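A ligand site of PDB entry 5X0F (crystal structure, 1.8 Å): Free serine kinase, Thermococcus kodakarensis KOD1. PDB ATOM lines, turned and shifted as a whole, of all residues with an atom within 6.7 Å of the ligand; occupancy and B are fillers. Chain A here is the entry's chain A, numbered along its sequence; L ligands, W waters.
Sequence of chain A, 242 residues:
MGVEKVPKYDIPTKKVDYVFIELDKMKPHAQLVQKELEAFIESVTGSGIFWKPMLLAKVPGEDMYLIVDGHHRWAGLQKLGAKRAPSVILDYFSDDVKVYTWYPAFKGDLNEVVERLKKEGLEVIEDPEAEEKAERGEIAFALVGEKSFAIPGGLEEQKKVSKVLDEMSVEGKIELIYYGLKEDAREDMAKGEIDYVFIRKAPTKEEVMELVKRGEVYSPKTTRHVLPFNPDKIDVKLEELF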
ATOM      1  N   GLU A  36     -17.940  17.541  -0.502  1.00  0.00           N
ATOM      2  CA  GLU A  36     -17.331  16.395   0.139  1.00  0.00           C
ATOM      3  C   GLU A  36     -17.211  15.252  -0.875  1.00  0.00           C
ATOM      4  O   GLU A  36     -16.262  14.500  -0.846  1.00  0.00           O
ATOM      5  CB  GLU A  36     -18.126  15.937   1.363  1.00  0.00           C
ATOM      6  CG  GLU A  36     -18.066  16.939   2.519  1.00  0.00           C
ATOM      7  CD  GLU A  36     -18.916  16.541   3.709  1.00  0.00           C
ATOM      8  OE1 GLU A  36     -18.920  15.352   4.082  1.00  0.00           O
ATOM      9  OE2 GLU A  36     -19.582  17.434   4.264  1.00  0.00           O
ATOM     10  N   LEU A  37     -18.223  15.135  -1.726  1.00  0.00           N
ATOM     11  CA  LEU A  37     -18.229  14.194  -2.835  1.00  0.00           C
ATOM     12  C   LEU A  37     -17.028  14.473  -3.772  1.00  0.00           C
ATOM     13  O   LEU A  37     -16.247  13.595  -4.082  1.00  0.00           O
ATOM     14  CB  LEU A  37     -19.566  14.368  -3.597  1.00  0.00           C
ATOM     15  CG  LEU A  37     -19.835  13.586  -4.881  1.00  0.00           C
ATOM     16  CD1 LEU A  37     -19.523  12.133  -4.644  1.00  0.00           C
ATOM     17  CD2 LEU A  37     -21.284  13.735  -5.325  1.00  0.00           C
ATOM     18  N   ALA A  39     -14.232  16.233  -3.119  1.00  0.00           N
ATOM     19  CA  ALA A  39     -12.944  15.993  -2.456  1.00  0.00           C
ATOM     20  C   ALA A  39     -12.577  14.499  -2.410  1.00  0.00           C
ATOM     21  O   ALA A  39     -11.419  14.128  -2.649  1.00  0.00           O
ATOM     22  CB  ALA A  39     -12.923  16.619  -1.067  1.00  0.00           C
ATOM     23  N   PHE A  40     -13.566  13.639  -2.146  1.00  0.00           N
ATOM     24  CA  PHE A  40     -13.315  12.195  -2.193  1.00  0.00           C
ATOM     25  C   PHE A  40     -12.865  11.760  -3.598  1.00  0.00           C
ATOM     26  O   PHE A  40     -11.876  11.012  -3.751  1.00  0.00           O
ATOM     27  CB  PHE A  40     -14.517  11.351  -1.709  1.00  0.00           C
ATOM     28  CG  PHE A  40     -14.346   9.904  -2.079  1.00  0.00           C
ATOM     29  CD1 PHE A  40     -13.417   9.123  -1.392  1.00  0.00           C
ATOM     30  CD2 PHE A  40     -15.025   9.342  -3.140  1.00  0.00           C
ATOM     31  CE1 PHE A  40     -13.185   7.803  -1.760  1.00  0.00           C
ATOM     32  CE2 PHE A  40     -14.770   8.030  -3.533  1.00  0.00           C
ATOM     33  CZ  PHE A  40     -13.871   7.246  -2.820  1.00  0.00           C
ATOM     34  N   SER A  43      -9.342  12.720  -4.303  1.00  0.00           N
ATOM     35  CA  SER A  43      -8.394  12.027  -3.456  1.00  0.00           C
ATOM     36  C   SER A  43      -8.209  10.591  -3.930  1.00  0.00           C
ATOM     37  O   SER A  43      -7.075  10.167  -4.078  1.00  0.00           O
ATOM     38  CB  SER A  43      -8.868  12.035  -1.991  1.00  0.00           C
ATOM     39  OG  SER A  43      -7.974  11.294  -1.128  1.00  0.00           O
ATOM     40  N   VAL A  44      -9.304   9.860  -4.175  1.00  0.00           N
ATOM     41  CA  VAL A  44      -9.174   8.452  -4.562  1.00  0.00           C
ATOM     42  C   VAL A  44      -8.574   8.290  -5.958  1.00  0.00           C
ATOM     43  O   VAL A  44      -7.770   7.387  -6.172  1.00  0.00           O
ATOM     44  CB  VAL A  44     -10.482   7.646  -4.412  1.00  0.00           C
ATOM     45  CG1 VAL A  44     -11.452   7.938  -5.524  1.00  0.00           C
ATOM     46  CG2 VAL A  44     -10.206   6.142  -4.316  1.00  0.00           C
ATOM     47  N   THR A  45      -8.942   9.159  -6.885  1.00  0.00           N
ATOM     48  CA  THR A  45      -8.374   9.115  -8.240  1.00  0.00           C
ATOM     49  C   THR A  45      -6.908   9.545  -8.198  1.00  0.00           C
ATOM     50  O   THR A  45      -6.129   9.098  -9.024  1.00  0.00           O
ATOM     51  CB  THR A  45      -9.157   9.959  -9.258  1.00  0.00           C
ATOM     52  OG1 THR A  45      -9.207  11.337  -8.869  1.00  0.00           O
ATOM     53  CG2 THR A  45     -10.594   9.433  -9.450  1.00  0.00           C
ATOM     54  N   SER A  47      -4.602   8.929  -5.703  1.00  0.00           N
ATOM     55  CA  SER A  47      -3.673   7.878  -5.210  1.00  0.00           C
ATOM     56  C   SER A  47      -3.943   6.550  -5.845  1.00  0.00           C
ATOM     57  O   SER A  47      -3.045   5.730  -5.967  1.00  0.00           O
ATOM     58  CB  SER A  47      -3.757   7.747  -3.697  1.00  0.00           C
ATOM     59  OG  SER A  47      -5.077   7.436  -3.325  1.00  0.00           O
ATOM     60  N   GLY A  48      -5.189   6.323  -6.249  1.00  0.00           N
ATOM     61  CA  GLY A  48      -5.621   5.011  -6.705  1.00  0.00           C
ATOM     62  C   GLY A  48      -5.707   3.969  -5.611  1.00  0.00           C
ATOM     63  O   GLY A  48      -5.746   2.772  -5.920  1.00  0.00           O
ATOM     64  N   ILE A  49      -5.744   4.390  -4.334  1.00  0.00           N
ATOM     65  CA  ILE A  49      -5.877   3.489  -3.174  1.00  0.00           C
ATOM     66  C   ILE A  49      -7.121   3.919  -2.417  1.00  0.00           C
ATOM     67  O   ILE A  49      -7.306   5.130  -2.193  1.00  0.00           O
ATOM     68  CB  ILE A  49      -4.674   3.639  -2.163  1.00  0.00           C
ATOM     69  CG1 ILE A  49      -3.360   3.321  -2.850  1.00  0.00           C
ATOM     70  CG2 ILE A  49      -4.913   2.837  -0.867  1.00  0.00           C
ATOM     71  CD1 ILE A  49      -3.222   1.950  -3.431  1.00  0.00           C
ATOM     72  N   PHE A  50      -7.949   2.955  -2.034  1.00  0.00           N
ATOM     73  CA  PHE A  50      -9.144   3.197  -1.225  1.00  0.00           C
ATOM     74  C   PHE A  50      -8.802   2.598   0.148  1.00  0.00           C
ATOM     75  O   PHE A  50      -8.700   1.403   0.251  1.00  0.00           O
ATOM     76  CB  PHE A  50     -10.389   2.543  -1.882  1.00  0.00           C
ATOM     77  CG  PHE A  50     -11.702   2.838  -1.177  1.00  0.00           C
ATOM     78  CD1 PHE A  50     -12.080   2.111  -0.029  1.00  0.00           C
ATOM     79  CD2 PHE A  50     -12.566   3.786  -1.633  1.00  0.00           C
ATOM     80  CE1 PHE A  50     -13.263   2.402   0.618  1.00  0.00           C
ATOM     81  CE2 PHE A  50     -13.751   4.090  -0.985  1.00  0.00           C
ATOM     82  CZ  PHE A  50     -14.107   3.397   0.163  1.00  0.00           C
ATOM     83  N   TRP A  51      -8.596   3.439   1.153  1.00  0.00           N
ATOM     84  CA  TRP A  51      -7.950   3.030   2.402  1.00  0.00           C
ATOM     85  C   TRP A  51      -8.841   3.010   3.642  1.00  0.00           C
ATOM     86  O   TRP A  51      -8.370   2.593   4.731  1.00  0.00           O
ATOM     87  CB  TRP A  51      -6.676   3.894   2.655  1.00  0.00           C
ATOM     88  CG  TRP A  51      -6.894   5.335   2.520  1.00  0.00           C
ATOM     89  CD1 TRP A  51      -6.491   6.119   1.455  1.00  0.00           C
ATOM     90  CD2 TRP A  51      -7.520   6.223   3.446  1.00  0.00           C
ATOM     91  NE1 TRP A  51      -6.827   7.432   1.690  1.00  0.00           N
ATOM     92  CE2 TRP A  51      -7.475   7.513   2.891  1.00  0.00           C
ATOM     93  CE3 TRP A  51      -8.100   6.068   4.710  1.00  0.00           C
ATOM     94  CZ2 TRP A  51      -8.008   8.620   3.535  1.00  0.00           C
ATOM     95  CZ3 TRP A  51      -8.610   7.184   5.370  1.00  0.00           C
ATOM     96  CH2 TRP A  51      -8.572   8.452   4.752  1.00  0.00           C
ATOM     97  N   LYS A  52     -10.128   3.371   3.486  1.00  0.00           N
ATOM     98  CA  LYS A  52     -11.074   3.672   4.598  1.00  0.00           C
ATOM     99  C   LYS A  52     -12.384   2.928   4.325  1.00  0.00           C
ATOM    100  O   LYS A  52     -13.238   3.380   3.555  1.00  0.00           O
ATOM    101  CB  LYS A  52     -11.373   5.198   4.716  1.00  0.00           C
ATOM    102  CG  LYS A  52     -12.039   5.655   6.055  1.00  0.00           C
ATOM    103  CD  LYS A  52     -12.404   7.150   6.059  1.00  0.00           C
ATOM    104  CE  LYS A  52     -12.620   7.777   7.436  1.00  0.00           C
ATOM    105  N   PRO A  53     -12.585   1.743   4.914  1.00  0.00           N
ATOM    106  CA  PRO A  53     -13.809   0.998   4.510  1.00  0.00           C
ATOM    107  C   PRO A  53     -15.105   1.694   4.927  1.00  0.00           C
ATOM    108  O   PRO A  53     -15.119   2.405   5.943  1.00  0.00           O
ATOM    109  CB  PRO A  53     -13.683  -0.339   5.301  1.00  0.00           C
ATOM    110  CG  PRO A  53     -12.820   0.031   6.468  1.00  0.00           C
ATOM    111  CD  PRO A  53     -11.831   1.028   5.963  1.00  0.00           C
ATOM    112  N   MET A  54     -16.157   1.484   4.156  1.00  0.00           N
ATOM    113  CA  MET A  54     -17.522   1.888   4.503  1.00  0.00           C
ATOM    114  C   MET A  54     -17.874   1.173   5.802  1.00  0.00           C
ATOM    115  O   MET A  54     -17.355   0.099   6.038  1.00  0.00           O
ATOM    116  CB  MET A  54     -18.536   1.382   3.476  1.00  0.00           C
ATOM    117  CG  MET A  54     -18.298   1.712   2.035  1.00  0.00           C
ATOM    118  SD  MET A  54     -18.769   3.389   1.753  1.00  0.00           S
ATOM    119  CE  MET A  54     -20.520   3.452   2.205  1.00  0.00           C
ATOM    120  N   ASP A  69     -21.531   5.029   7.857  1.00  0.00           N
ATOM    121  CA  ASP A  69     -20.468   5.994   7.559  1.00  0.00           C
ATOM    122  C   ASP A  69     -19.923   5.666   6.188  1.00  0.00           C
ATOM    123  O   ASP A  69     -19.588   4.520   5.900  1.00  0.00           O
ATOM    124  CB  ASP A  69     -19.351   5.929   8.646  1.00  0.00           C
ATOM    125  CG  ASP A  69     -18.310   7.022   8.489  1.00  0.00           C
ATOM    126  OD1 ASP A  69     -18.688   8.189   8.532  1.00  0.00           O
ATOM    127  OD2 ASP A  69     -17.118   6.701   8.259  1.00  0.00           O
ATOM    128  N   GLY A  70     -19.846   6.697   5.351  1.00  0.00           N
ATOM    129  CA  GLY A  70     -19.369   6.522   3.990  1.00  0.00           C
ATOM    130  C   GLY A  70     -20.236   7.093   2.887  1.00  0.00           C
ATOM    131  O   GLY A  70     -20.052   6.650   1.742  1.00  0.00           O
ATOM    132  N   HIS A  71     -21.122   8.041   3.144  1.00  0.00           N
ATOM    133  CA  HIS A  71     -22.005   8.540   2.067  1.00  0.00           C
ATOM    134  C   HIS A  71     -21.279   9.055   0.813  1.00  0.00           C
ATOM    135  O   HIS A  71     -21.700   8.776  -0.322  1.00  0.00           O
ATOM    136  CB  HIS A  71     -22.949   9.617   2.556  1.00  0.00           C
ATOM    137  CG  HIS A  71     -24.007   9.110   3.490  1.00  0.00           C
ATOM    138  ND1 HIS A  71     -23.995   9.415   4.825  1.00  0.00           N
ATOM    139  CD2 HIS A  71     -25.113   8.363   3.287  1.00  0.00           C
ATOM    140  CE1 HIS A  71     -25.027   8.846   5.428  1.00  0.00           C
ATOM    141  NE2 HIS A  71     -25.725   8.216   4.506  1.00  0.00           N
ATOM    142  N   HIS A  72     -20.223   9.835   1.020  1.00  0.00           N
ATOM    143  CA  HIS A  72     -19.487  10.443  -0.113  1.00  0.00           C
ATOM    144  C   HIS A  72     -18.520   9.513  -0.827  1.00  0.00           C
ATOM    145  O   HIS A  72     -18.346   9.617  -2.043  1.00  0.00           O
ATOM    146  CB  HIS A  72     -18.869  11.750   0.314  1.00  0.00           C
ATOM    147  CG  HIS A  72     -19.865  12.695   0.892  1.00  0.00           C
ATOM    148  ND1 HIS A  72     -20.176  12.700   2.241  1.00  0.00           N
ATOM    149  CD2 HIS A  72     -20.719  13.562   0.312  1.00  0.00           C
ATOM    150  CE1 HIS A  72     -21.126  13.581   2.473  1.00  0.00           C
ATOM    151  NE2 HIS A  72     -21.473  14.117   1.320  1.00  0.00           N
ATOM    152  N   ARG A  73     -17.916   8.577  -0.089  1.00  0.00           N
ATOM    153  CA  ARG A  73     -17.251   7.432  -0.703  1.00  0.00           C
ATOM    154  C   ARG A  73     -18.186   6.647  -1.613  1.00  0.00           C
ATOM    155  O   ARG A  73     -17.874   6.383  -2.775  1.00  0.00           O
ATOM    156  CB  ARG A  73     -16.678   6.477   0.367  1.00  0.00           C
ATOM    157  CG  ARG A  73     -15.357   6.970   0.929  1.00  0.00           C
ATOM    158  CD  ARG A  73     -15.068   6.273   2.261  1.00  0.00           C
ATOM    159  NE  ARG A  73     -15.764   6.901   3.389  1.00  0.00           N
ATOM    160  CZ  ARG A  73     -15.864   6.352   4.612  1.00  0.00           C
ATOM    161  NH1 ARG A  73     -15.282   5.213   4.879  1.00  0.00           N
ATOM    162  NH2 ARG A  73     -16.479   7.018   5.583  1.00  0.00           N
ATOM    163  N   TRP A  74     -19.348   6.283  -1.084  1.00  0.00           N
ATOM    164  CA  TRP A  74     -20.368   5.583  -1.885  1.00  0.00           C
ATOM    165  C   TRP A  74     -20.757   6.373  -3.135  1.00  0.00           C
ATOM    166  O   TRP A  74     -20.690   5.852  -4.243  1.00  0.00           O
ATOM    167  CB  TRP A  74     -21.617   5.322  -1.029  1.00  0.00           C
ATOM    168  CG  TRP A  74     -22.858   4.831  -1.750  1.00  0.00           C
ATOM    169  CD1 TRP A  74     -23.099   3.608  -2.226  1.00  0.00           C
ATOM    170  CD2 TRP A  74     -24.040   5.601  -1.986  1.00  0.00           C
ATOM    171  NE1 TRP A  74     -24.345   3.545  -2.807  1.00  0.00           N
ATOM    172  CE2 TRP A  74     -24.966   4.758  -2.637  1.00  0.00           C
ATOM    173  CE3 TRP A  74     -24.406   6.900  -1.695  1.00  0.00           C
ATOM    174  CZ2 TRP A  74     -26.226   5.191  -3.047  1.00  0.00           C
ATOM    175  CZ3 TRP A  74     -25.703   7.345  -2.086  1.00  0.00           C
ATOM    176  CH2 TRP A  74     -26.583   6.483  -2.749  1.00  0.00           C
HETATM  177  P1  LIG L   1     -17.745  10.109   3.752  1.00  0.00           P
HETATM  178  O1  LIG L   1     -17.637   8.975   2.763  1.00  0.00           O
HETATM  179  O2  LIG L   1     -19.071  10.816   3.817  1.00  0.00           O
HETATM  180  O3  LIG L   1     -17.172   9.752   5.104  1.00  0.00           O
HETATM  181  O4  LIG L   1     -16.780  11.277   3.148  1.00  0.00           O
HETATM  182  C1  LIG L   1     -15.674  10.972   2.310  1.00  0.00           C
HETATM  183  C2  LIG L   1     -14.583  10.240   3.051  1.00  0.00           C
HETATM  184  O5  LIG L   1     -13.607   9.780   2.120  1.00  0.00           O
HETATM  185  C3  LIG L   1     -13.812  11.089   4.064  1.00  0.00           C
HETATM  186  O6  LIG L   1     -14.047  10.609   5.394  1.00  0.00           O
HETATM  187  C4  LIG L   1     -12.355  10.912   3.722  1.00  0.00           C
HETATM  188  O7  LIG L   1     -11.506  10.569   4.833  1.00  0.00           O
HETATM  189  C5  LIG L   1     -12.397   9.678   2.834  1.00  0.00           C
HETATM  190  N1  LIG L   1     -11.310   9.503   1.881  1.00  0.00           N
HETATM  191  C6  LIG L   1     -10.512  10.446   1.307  1.00  0.00           C
HETATM  192  N2  LIG L   1      -9.662   9.843   0.448  1.00  0.00           N
HETATM  193  C7  LIG L   1      -9.923   8.525   0.438  1.00  0.00           C
HETATM  194  C8  LIG L   1      -9.405   7.332  -0.232  1.00  0.00           C
HETATM  195  N3  LIG L   1      -8.383   7.419  -1.122  1.00  0.00           N
HETATM  196  N4  LIG L   1      -9.978   6.123   0.061  1.00  0.00           N
HETATM  197  C9  LIG L   1     -11.007   6.016   0.930  1.00  0.00           C
HETATM  198  N5  LIG L   1     -11.525   7.065   1.595  1.00  0.00           N
HETATM  199  C10 LIG L   1     -11.016   8.307   1.390  1.00  0.00           C
HETATM  200  O   HOH W   1     -20.958   9.325   5.707  1.00  0.00           O
HETATM  201  O   HOH W   2     -20.181  12.750   5.668  1.00  0.00           O
HETATM  202  O   HOH W   3     -10.350   9.592   7.804  1.00  0.00           O
HETATM  203  O   HOH W   4     -16.702  13.847   4.083  1.00  0.00           O
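The backbone NH of His 72 lies within hydrogen-bond range of an oxygen (O2) of the ligand.
A ring nitrogen (ND1) of His 72 sits at hydrogen-bond distance from an oxygen (O2) of the ligand, 2.7 Å away.
The side-chain hydroxyl (OG) of Ser 43 is in hydrogen-bond range of a nitrogen (N2) of the ligand (2.7 Å).
O of Ile 49 lies within hydrogen-bond range of N3 of the ligand (2.7 Å).
The backbone NH (N) of Arg 73 sits at hydrogen-bond distance from an oxygen (O1) of the ligand (2.9 Å).
An oxygen (O3) of the ligand is in salt-bridge range of the guanidinium group (NH2) of Arg 73, at 2.9 Å.
N4 of the ligand is in hydrogen-bond range of N of Trp 51.
Water W4 bridges the side-chain carboxylate (OE1) of Glu 36 (2.7 Å) and an oxygen (O4) of the ligand (2.7 Å).
Water W2 lies within hydrogen-bond range of O2 of the ligand (2.9 Å), OE1 of Glu 36 (3.3 Å) and ND1 of His 72 (3.4 Å).
Water W1 lies within hydrogen-bond range of the backbone NH of His 71 (2.9 Å), the backbone NH of Gly 70 (2.9 Å) and an oxygen (O2) of the ligand (3.1 Å).
Merely in contact with the ligand: Gly 70, Phe 50, His 71, Phe 40, Lys 52, Val 44 and Ser 47.
12 residues have an atom within 4 Å of the ligand: Phe 40, Ser 43, Val 44, Ser 47, Ile 49, Phe 50, Trp 51, Lys 52, Gly 70, His 71, His 72 and Arg 73.
The nearest printed residue that does not touch the ligand is Asp 69 (4.1 Å).
The side-chain carboxylate (OE1) of Glu 36 lies close to a ring nitrogen (ND1) of His 72 (3.5 Å).
The side-chain hydroxyl of Ser 47 is in hydrogen-bond range of the backbone carbonyl oxygen of Ser 43 (3.5 Å).
N of Ile 49 sits close to OG of Ser 47 (3.3 Å).
NH1 of Arg 73 sits at hydrogen-bond distance from O of Lys 52.
NH2 of Arg 73 is in salt-bridge range of OD2 of Asp 69 (2.8 Å).
The backbone carbonyl oxygen of Pro 53 lies within hydrogen-bond range of the guanidinium group of Arg 73.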
